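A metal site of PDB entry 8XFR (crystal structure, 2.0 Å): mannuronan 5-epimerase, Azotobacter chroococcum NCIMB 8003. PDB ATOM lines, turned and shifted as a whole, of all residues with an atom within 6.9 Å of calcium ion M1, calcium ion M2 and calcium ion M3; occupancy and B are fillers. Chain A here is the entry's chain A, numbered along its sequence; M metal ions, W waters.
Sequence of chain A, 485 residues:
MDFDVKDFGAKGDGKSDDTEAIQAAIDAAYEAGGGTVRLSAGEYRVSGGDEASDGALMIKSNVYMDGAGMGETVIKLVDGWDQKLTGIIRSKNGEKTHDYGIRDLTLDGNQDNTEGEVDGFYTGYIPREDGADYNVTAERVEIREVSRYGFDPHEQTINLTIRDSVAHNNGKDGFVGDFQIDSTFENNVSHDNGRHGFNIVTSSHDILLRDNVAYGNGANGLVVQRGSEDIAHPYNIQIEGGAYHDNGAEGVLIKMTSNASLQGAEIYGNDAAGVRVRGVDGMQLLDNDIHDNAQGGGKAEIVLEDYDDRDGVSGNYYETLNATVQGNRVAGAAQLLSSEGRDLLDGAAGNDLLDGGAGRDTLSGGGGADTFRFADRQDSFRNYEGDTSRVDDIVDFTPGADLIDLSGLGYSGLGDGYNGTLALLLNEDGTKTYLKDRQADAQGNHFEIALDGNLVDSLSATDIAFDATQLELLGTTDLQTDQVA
Calcium ion M1 is bound by the backbone carbonyl oxygen (O) of Ala 358 (2.3 Å), the backbone carbonyl oxygen (O) of Gly 341 (2.3 Å), the backbone carbonyl oxygen (O) of Gly 356 (2.4 Å), the side-chain carboxylate (OD2) of Asp 343 (2.4 Å), the backbone carbonyl oxygen (O) of Ser 339 (2.4 Å) and the side-chain carboxylate (OD1) of Asp 361 (2.4 Å).
Slightly farther from calcium ion M1 lies OD2 of Asp 361 (2.9 Å).
Residues that only touch calcium ion M3: Asp 376 (2.9 Å).
Of the 28 residues printed, 6 come within 4 Å of calcium ion M2.
Within 4 Å of calcium ion M1: Ser 339, Gly 341, Asp 343, Gly 356, Ala 358 and Asp 361.
The side-chain hydroxyl of Ser 338 lies within hydrogen-bond range of the side-chain carboxylate of Asp 343 (2.6 Å).
The backbone carbonyl oxygen (O) of Asp 343 is in hydrogen-bond range of the backbone NH (N) of Thr 362, at 3.0 Å.
The backbone NH of Gly 357 sits close to the backbone carbonyl oxygen of Ser 338, 3.4 Å away.
N of Asp 392 lies within hydrogen-bond range of OG of Ser 380, 2.8 Å away.
The backbone NH (N) of Ala 358 sits close to the side-chain carboxylate (OD1) of Asp 379, at 3.5 Å.
The backbone NH (N) of Gln 378 lies within hydrogen-bond range of the side-chain carboxylate (OD1) of Asp 376, 2.7 Å away.
N of Gly 357 is in hydrogen-bond range of OD1 of Asp 355 (2.8 Å).
OD1 of Asp 343 sits at hydrogen-bond distance from N of Asn 322, 3.4 Å away.
Calcium ion M2 is bound by the backbone carbonyl oxygen (O) of Asp 379 (2.3 Å).
Calcium ion M2 is bound by the backbone carbonyl oxygen (O) of Gly 359 (2.4 Å).
OD2 of Asp 361 is bound to calcium ion M2.
The side-chain carboxylate (OD1) of Asp 392 binds calcium ion M2 (2.4 Å).
The backbone carbonyl oxygen (O) of Gly 357 binds calcium ion M2 (2.5 Å).
Calcium ion M2 is bound by water W2.
OD2 of Asp 392 is bound to calcium ion M2.
Calcium ion M3 is bound by water W3 (2.4 Å).
Water W1 is bound to calcium ion M3, at 2.4 Å.
Calcium ion M3 is bound by OD1 of Asp 379, at 2.6 Å.
Slightly farther from calcium ion M3 lies OD2 of Asp 379 (3.0 Å).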
ATOM      1  N   ASN A 322       5.560 -34.144  -6.994  1.00  0.00           N
ATOM      2  CA  ASN A 322       6.722 -34.590  -6.218  1.00  0.00           C
ATOM      3  C   ASN A 322       7.551 -35.610  -6.979  1.00  0.00           C
ATOM      4  O   ASN A 322       7.856 -36.689  -6.490  1.00  0.00           O
ATOM      5  CB  ASN A 322       6.266 -35.160  -4.883  1.00  0.00           C
ATOM      6  CG  ASN A 322       5.600 -34.102  -4.027  1.00  0.00           C
ATOM      7  OD1 ASN A 322       6.114 -32.970  -3.922  1.00  0.00           O
ATOM      8  ND2 ASN A 322       4.395 -34.417  -3.501  1.00  0.00           N
ATOM      9  N   SER A 338       5.090 -32.037 -14.304  1.00  0.00           N
ATOM     10  CA  SER A 338       4.657 -32.196 -12.915  1.00  0.00           C
ATOM     11  C   SER A 338       3.894 -30.938 -12.500  1.00  0.00           C
ATOM     12  O   SER A 338       3.702 -30.015 -13.294  1.00  0.00           O
ATOM     13  CB  SER A 338       5.851 -32.504 -12.008  1.00  0.00           C
ATOM     14  OG  SER A 338       5.391 -33.015 -10.768  1.00  0.00           O
ATOM     15  N   SER A 339       3.536 -30.863 -11.216  1.00  0.00           N
ATOM     16  CA  SER A 339       2.598 -29.855 -10.724  1.00  0.00           C
ATOM     17  C   SER A 339       3.141 -29.295  -9.406  1.00  0.00           C
ATOM     18  O   SER A 339       4.352 -29.265  -9.174  1.00  0.00           O
ATOM     19  CB  SER A 339       1.199 -30.460 -10.631  1.00  0.00           C
ATOM     20  OG  SER A 339       0.659 -30.670 -11.930  1.00  0.00           O
ATOM     21  N   GLU A 340       2.237 -28.738  -8.587  1.00  0.00           N
ATOM     22  CA  GLU A 340       2.581 -28.015  -7.361  1.00  0.00           C
ATOM     23  C   GLU A 340       3.625 -28.775  -6.501  1.00  0.00           C
ATOM     24  O   GLU A 340       3.587 -30.009  -6.391  1.00  0.00           O
ATOM     25  CB  GLU A 340       1.331 -27.755  -6.531  1.00  0.00           C
ATOM     26  CG  GLU A 340       1.648 -27.041  -5.186  1.00  0.00           C
ATOM     27  CD  GLU A 340       2.342 -25.663  -5.357  1.00  0.00           C
ATOM     28  OE1 GLU A 340       1.607 -24.653  -5.511  1.00  0.00           O
ATOM     29  OE2 GLU A 340       3.617 -25.582  -5.371  1.00  0.00           O
ATOM     30  N   GLY A 341       4.546 -28.021  -5.911  1.00  0.00           N
ATOM     31  CA  GLY A 341       5.645 -28.601  -5.155  1.00  0.00           C
ATOM     32  C   GLY A 341       6.929 -28.660  -5.985  1.00  0.00           C
ATOM     33  O   GLY A 341       6.940 -28.420  -7.194  1.00  0.00           O
ATOM     34  N   ARG A 342       8.019 -29.007  -5.311  1.00  0.00           N
ATOM     35  CA  ARG A 342       9.339 -28.971  -5.930  1.00  0.00           C
ATOM     36  C   ARG A 342       9.573 -30.245  -6.728  1.00  0.00           C
ATOM     37  O   ARG A 342       9.510 -31.348  -6.172  1.00  0.00           O
ATOM     38  CB  ARG A 342      10.421 -28.822  -4.854  1.00  0.00           C
ATOM     39  CG  ARG A 342      11.837 -28.979  -5.351  1.00  0.00           C
ATOM     40  CD  ARG A 342      12.772 -28.045  -4.548  1.00  0.00           C
ATOM     41  NE  ARG A 342      14.163 -28.228  -4.939  1.00  0.00           N
ATOM     42  CZ  ARG A 342      14.700 -27.744  -6.059  1.00  0.00           C
ATOM     43  NH1 ARG A 342      13.968 -27.049  -6.922  1.00  0.00           N
ATOM     44  NH2 ARG A 342      15.996 -27.945  -6.293  1.00  0.00           N
ATOM     45  N   ASP A 343       9.850 -30.101  -8.021  1.00  0.00           N
ATOM     46  CA  ASP A 343      10.229 -31.214  -8.874  1.00  0.00           C
ATOM     47  C   ASP A 343      11.652 -31.016  -9.358  1.00  0.00           C
ATOM     48  O   ASP A 343      12.106 -29.892  -9.520  1.00  0.00           O
ATOM     49  CB  ASP A 343       9.272 -31.289 -10.086  1.00  0.00           C
ATOM     50  CG  ASP A 343       7.848 -31.536  -9.642  1.00  0.00           C
ATOM     51  OD1 ASP A 343       7.535 -32.717  -9.362  1.00  0.00           O
ATOM     52  OD2 ASP A 343       7.048 -30.576  -9.536  1.00  0.00           O
ATOM     53  N   LEU A 345      13.625 -32.391 -12.585  1.00  0.00           N
ATOM     54  CA  LEU A 345      13.349 -33.080 -13.843  1.00  0.00           C
ATOM     55  C   LEU A 345      14.570 -32.939 -14.743  1.00  0.00           C
ATOM     56  O   LEU A 345      14.892 -31.830 -15.176  1.00  0.00           O
ATOM     57  CB  LEU A 345      12.089 -32.504 -14.510  1.00  0.00           C
ATOM     58  CG  LEU A 345      10.844 -32.484 -13.605  1.00  0.00           C
ATOM     59  CD1 LEU A 345       9.658 -31.738 -14.261  1.00  0.00           C
ATOM     60  CD2 LEU A 345      10.406 -33.911 -13.258  1.00  0.00           C
ATOM     61  N   ASP A 355       8.327 -29.522 -17.861  1.00  0.00           N
ATOM     62  CA  ASP A 355       7.441 -28.543 -17.237  1.00  0.00           C
ATOM     63  C   ASP A 355       7.231 -28.969 -15.799  1.00  0.00           C
ATOM     64  O   ASP A 355       6.476 -29.896 -15.532  1.00  0.00           O
ATOM     65  CB  ASP A 355       6.101 -28.460 -17.973  1.00  0.00           C
ATOM     66  CG  ASP A 355       5.245 -27.255 -17.513  1.00  0.00           C
ATOM     67  OD1 ASP A 355       5.511 -26.652 -16.429  1.00  0.00           O
ATOM     68  OD2 ASP A 355       4.298 -26.893 -18.262  1.00  0.00           O
ATOM     69  N   GLY A 356       7.846 -28.250 -14.873  1.00  0.00           N
ATOM     70  CA  GLY A 356       7.572 -28.574 -13.487  1.00  0.00           C
ATOM     71  C   GLY A 356       6.288 -27.994 -12.908  1.00  0.00           C
ATOM     72  O   GLY A 356       5.966 -28.300 -11.759  1.00  0.00           O
ATOM     73  N   GLY A 357       5.525 -27.191 -13.657  1.00  0.00           N
ATOM     74  CA  GLY A 357       4.271 -26.718 -13.078  1.00  0.00           C
ATOM     75  C   GLY A 357       4.505 -25.737 -11.929  1.00  0.00           C
ATOM     76  O   GLY A 357       5.530 -25.070 -11.845  1.00  0.00           O
ATOM     77  N   ALA A 358       3.541 -25.650 -11.007  1.00  0.00           N
ATOM     78  CA  ALA A 358       3.715 -24.757  -9.879  1.00  0.00           C
ATOM     79  C   ALA A 358       4.860 -25.232  -8.982  1.00  0.00           C
ATOM     80  O   ALA A 358       5.323 -26.372  -9.061  1.00  0.00           O
ATOM     81  CB  ALA A 358       2.414 -24.631  -9.088  1.00  0.00           C
ATOM     82  N   GLY A 359       5.364 -24.318  -8.145  1.00  0.00           N
ATOM     83  CA  GLY A 359       6.451 -24.630  -7.231  1.00  0.00           C
ATOM     84  C   GLY A 359       7.838 -24.371  -7.813  1.00  0.00           C
ATOM     85  O   GLY A 359       8.024 -24.125  -9.004  1.00  0.00           O
ATOM     86  N   ARG A 360       8.845 -24.465  -6.937  1.00  0.00           N
ATOM     87  CA  ARG A 360      10.234 -24.206  -7.306  1.00  0.00           C
ATOM     88  C   ARG A 360      10.867 -25.456  -7.886  1.00  0.00           C
ATOM     89  O   ARG A 360      11.220 -26.389  -7.151  1.00  0.00           O
ATOM     90  CB  ARG A 360      11.037 -23.716  -6.094  1.00  0.00           C
ATOM     91  CG  ARG A 360      12.392 -23.160  -6.508  1.00  0.00           C
ATOM     92  CD  ARG A 360      13.178 -22.603  -5.322  1.00  0.00           C
ATOM     93  NE  ARG A 360      13.696 -23.647  -4.443  1.00  0.00           N
ATOM     94  CZ  ARG A 360      14.801 -24.358  -4.653  1.00  0.00           C
ATOM     95  NH1 ARG A 360      15.563 -24.159  -5.723  1.00  0.00           N
ATOM     96  NH2 ARG A 360      15.140 -25.292  -3.770  1.00  0.00           N
ATOM     97  N   ASP A 361      11.031 -25.492  -9.207  1.00  0.00           N
ATOM     98  CA  ASP A 361      11.521 -26.684  -9.877  1.00  0.00           C
ATOM     99  C   ASP A 361      12.912 -26.452 -10.436  1.00  0.00           C
ATOM    100  O   ASP A 361      13.279 -25.335 -10.810  1.00  0.00           O
ATOM    101  CB  ASP A 361      10.556 -27.080 -11.005  1.00  0.00           C
ATOM    102  CG  ASP A 361       9.142 -27.201 -10.509  1.00  0.00           C
ATOM    103  OD1 ASP A 361       8.910 -27.944  -9.541  1.00  0.00           O
ATOM    104  OD2 ASP A 361       8.256 -26.514 -11.028  1.00  0.00           O
ATOM    105  N   THR A 362      13.691 -27.521 -10.489  1.00  0.00           N
ATOM    106  CA  THR A 362      14.991 -27.482 -11.131  1.00  0.00           C
ATOM    107  C   THR A 362      14.945 -28.409 -12.341  1.00  0.00           C
ATOM    108  O   THR A 362      14.662 -29.600 -12.193  1.00  0.00           O
ATOM    109  CB  THR A 362      16.087 -27.888 -10.149  1.00  0.00           C
ATOM    110  OG1 THR A 362      16.107 -26.930  -9.070  1.00  0.00           O
ATOM    111  CG2 THR A 362      17.429 -27.906 -10.842  1.00  0.00           C
ATOM    112  N   LEU A 363      15.254 -27.867 -13.515  1.00  0.00           N
ATOM    113  CA  LEU A 363      15.104 -28.579 -14.777  1.00  0.00           C
ATOM    114  C   LEU A 363      16.426 -28.618 -15.513  1.00  0.00           C
ATOM    115  O   LEU A 363      17.191 -27.648 -15.497  1.00  0.00           O
ATOM    116  CB  LEU A 363      14.053 -27.921 -15.682  1.00  0.00           C
ATOM    117  CG  LEU A 363      12.781 -27.421 -14.992  1.00  0.00           C
ATOM    118  CD1 LEU A 363      12.066 -26.369 -15.835  1.00  0.00           C
ATOM    119  CD2 LEU A 363      11.835 -28.580 -14.743  1.00  0.00           C
ATOM    120  N   PHE A 374       6.796 -23.075 -19.575  1.00  0.00           N
ATOM    121  CA  PHE A 374       6.200 -22.391 -18.434  1.00  0.00           C
ATOM    122  C   PHE A 374       4.803 -22.013 -18.861  1.00  0.00           C
ATOM    123  O   PHE A 374       4.625 -21.115 -19.695  1.00  0.00           O
ATOM    124  CB  PHE A 374       7.046 -21.195 -18.019  1.00  0.00           C
ATOM    125  CG  PHE A 374       8.409 -21.595 -17.614  1.00  0.00           C
ATOM    126  CD1 PHE A 374       9.379 -21.841 -18.578  1.00  0.00           C
ATOM    127  CD2 PHE A 374       8.702 -21.830 -16.284  1.00  0.00           C
ATOM    128  CE1 PHE A 374      10.620 -22.260 -18.217  1.00  0.00           C
ATOM    129  CE2 PHE A 374       9.939 -22.255 -15.916  1.00  0.00           C
ATOM    130  CZ  PHE A 374      10.910 -22.477 -16.874  1.00  0.00           C
ATOM    131  N   ALA A 375       3.832 -22.748 -18.335  1.00  0.00           N
ATOM    132  CA  ALA A 375       2.446 -22.654 -18.777  1.00  0.00           C
ATOM    133  C   ALA A 375       1.660 -21.569 -18.079  1.00  0.00           C
ATOM    134  O   ALA A 375       0.566 -21.235 -18.540  1.00  0.00           O
ATOM    135  CB  ALA A 375       1.753 -23.999 -18.537  1.00  0.00           C
ATOM    136  N   ASP A 376       2.172 -21.001 -16.984  1.00  0.00           N
ATOM    137  CA  ASP A 376       1.419 -20.113 -16.119  1.00  0.00           C
ATOM    138  C   ASP A 376       2.406 -19.153 -15.463  1.00  0.00           C
ATOM    139  O   ASP A 376       3.496 -19.566 -15.056  1.00  0.00           O
ATOM    140  CB  ASP A 376       0.639 -20.931 -15.072  1.00  0.00           C
ATOM    141  CG  ASP A 376      -0.330 -20.108 -14.283  1.00  0.00           C
ATOM    142  OD1 ASP A 376       0.084 -19.167 -13.559  1.00  0.00           O
ATOM    143  OD2 ASP A 376      -1.521 -20.401 -14.367  1.00  0.00           O
ATOM    144  N   ARG A 377       2.028 -17.881 -15.356  1.00  0.00           N
ATOM    145  CA  ARG A 377       2.927 -16.902 -14.749  1.00  0.00           C
ATOM    146  C   ARG A 377       3.219 -17.218 -13.288  1.00  0.00           C
ATOM    147  O   ARG A 377       4.257 -16.793 -12.759  1.00  0.00           O
ATOM    148  CB  ARG A 377       2.324 -15.495 -14.869  1.00  0.00           C
ATOM    149  CG  ARG A 377       2.583 -14.827 -16.208  1.00  0.00           C
ATOM    150  CD  ARG A 377       1.848 -13.490 -16.335  1.00  0.00           C
ATOM    151  NE  ARG A 377       1.944 -12.990 -17.706  1.00  0.00           N
ATOM    152  CZ  ARG A 377       1.997 -11.708 -18.052  1.00  0.00           C
ATOM    153  NH1 ARG A 377       1.978 -10.746 -17.147  1.00  0.00           N
ATOM    154  NH2 ARG A 377       2.072 -11.391 -19.346  1.00  0.00           N
ATOM    155  N   GLN A 378       2.342 -17.966 -12.619  1.00  0.00           N
ATOM    156  CA  GLN A 378       2.541 -18.334 -11.240  1.00  0.00           C
ATOM    157  C   GLN A 378       3.325 -19.642 -11.090  1.00  0.00           C
ATOM    158  O   GLN A 378       3.434 -20.172  -9.980  1.00  0.00           O
ATOM    159  CB  GLN A 378       1.178 -18.451 -10.528  1.00  0.00           C
ATOM    160  CG  GLN A 378       0.380 -17.142 -10.403  1.00  0.00           C
ATOM    161  CD  GLN A 378       1.176 -15.965  -9.833  1.00  0.00           C
ATOM    162  OE1 GLN A 378       1.651 -16.012  -8.670  1.00  0.00           O
ATOM    163  NE2 GLN A 378       1.333 -14.901 -10.637  1.00  0.00           N
ATOM    164  N   ASP A 379       3.878 -20.170 -12.170  1.00  0.00           N
ATOM    165  CA  ASP A 379       4.640 -21.401 -12.054  1.00  0.00           C
ATOM    166  C   ASP A 379       6.103 -21.156 -11.714  1.00  0.00           C
ATOM    167  O   ASP A 379       6.792 -22.106 -11.325  1.00  0.00           O
ATOM    168  CB  ASP A 379       4.533 -22.186 -13.352  1.00  0.00           C
ATOM    169  CG  ASP A 379       3.138 -22.828 -13.527  1.00  0.00           C
ATOM    170  OD1 ASP A 379       2.322 -22.777 -12.564  1.00  0.00           O
ATOM    171  OD2 ASP A 379       2.873 -23.367 -14.599  1.00  0.00           O
ATOM    172  N   SER A 380       6.563 -19.912 -11.817  1.00  0.00           N
ATOM    173  CA  SER A 380       7.951 -19.543 -11.517  1.00  0.00           C
ATOM    174  C   SER A 380       7.922 -18.056 -11.232  1.00  0.00           C
ATOM    175  O   SER A 380       7.683 -17.279 -12.157  1.00  0.00           O
ATOM    176  CB  SER A 380       8.877 -19.879 -12.693  1.00  0.00           C
ATOM    177  OG  SER A 380      10.252 -19.748 -12.355  1.00  0.00           O
ATOM    178  N   PHE A 381       8.110 -17.660  -9.967  1.00  0.00           N
ATOM    179  CA  PHE A 381       7.834 -16.282  -9.560  1.00  0.00           C
ATOM    180  C   PHE A 381       8.553 -15.922  -8.263  1.00  0.00           C
ATOM    181  O   PHE A 381       8.909 -16.776  -7.447  1.00  0.00           O
ATOM    182  CB  PHE A 381       6.322 -16.047  -9.406  1.00  0.00           C
ATOM    183  CG  PHE A 381       5.733 -16.639  -8.150  1.00  0.00           C
ATOM    184  CD1 PHE A 381       5.331 -17.974  -8.117  1.00  0.00           C
ATOM    185  CD2 PHE A 381       5.568 -15.869  -7.005  1.00  0.00           C
ATOM    186  CE1 PHE A 381       4.790 -18.521  -6.966  1.00  0.00           C
ATOM    187  CE2 PHE A 381       5.023 -16.421  -5.847  1.00  0.00           C
ATOM    188  CZ  PHE A 381       4.638 -17.750  -5.827  1.00  0.00           C
ATOM    189  N   ARG A 390      10.276 -20.317  -5.054  1.00  0.00           N
ATOM    190  CA  ARG A 390       9.276 -20.440  -6.104  1.00  0.00           C
ATOM    191  C   ARG A 390       9.805 -19.969  -7.465  1.00  0.00           C
ATOM    192  O   ARG A 390       9.047 -19.978  -8.426  1.00  0.00           O
ATOM    193  CB  ARG A 390       7.968 -19.701  -5.775  1.00  0.00           C
ATOM    194  CG  ARG A 390       7.306 -19.998  -4.403  1.00  0.00           C
ATOM    195  CD  ARG A 390       7.378 -21.440  -3.906  1.00  0.00           C
ATOM    196  NE  ARG A 390       8.531 -21.749  -3.067  1.00  0.00           N
ATOM    197  CZ  ARG A 390       8.715 -21.285  -1.833  1.00  0.00           C
ATOM    198  NH1 ARG A 390       7.923 -20.361  -1.313  1.00  0.00           N
ATOM    199  NH2 ARG A 390       9.727 -21.759  -1.110  1.00  0.00           N
ATOM    200  N   VAL A 391      11.072 -19.598  -7.585  1.00  0.00           N
ATOM    201  CA  VAL A 391      11.672 -19.339  -8.897  1.00  0.00           C
ATOM    202  C   VAL A 391      12.349 -20.605  -9.423  1.00  0.00           C
ATOM    203  O   VAL A 391      13.290 -21.119  -8.802  1.00  0.00           O
ATOM    204  CB  VAL A 391      12.641 -18.151  -8.855  1.00  0.00           C
ATOM    205  CG1 VAL A 391      13.348 -17.994 -10.203  1.00  0.00           C
ATOM    206  CG2 VAL A 391      11.861 -16.875  -8.520  1.00  0.00           C
ATOM    207  N   ASP A 392      11.891 -21.090 -10.575  1.00  0.00           N
ATOM    208  CA  ASP A 392      12.523 -22.233 -11.238  1.00  0.00           C
ATOM    209  C   ASP A 392      13.934 -21.890 -11.694  1.00  0.00           C
ATOM    210  O   ASP A 392      14.220 -20.751 -12.067  1.00  0.00           O
ATOM    211  CB  ASP A 392      11.736 -22.643 -12.488  1.00  0.00           C
ATOM    212  CG  ASP A 392      10.415 -23.317 -12.180  1.00  0.00           C
ATOM    213  OD1 ASP A 392      10.057 -23.439 -10.986  1.00  0.00           O
ATOM    214  OD2 ASP A 392       9.769 -23.758 -13.149  1.00  0.00           O
HETATM  215 CA    CA M   1       6.519 -28.264  -9.466  1.00  0.00          CA
HETATM  216 CA    CA M   2       7.794 -24.193 -11.351  1.00  0.00          CA
HETATM  217 CA    CA M   3       0.005 -23.382 -13.642  1.00  0.00          CA
HETATM  218  O   HOH W   1      -0.366 -24.119 -11.420  1.00  0.00           O
HETATM  219  O   HOH W   2       7.318 -24.079 -13.788  1.00  0.00           O
HETATM  220  O   HOH W   3       0.637 -25.141 -15.093  1.00  0.00           O
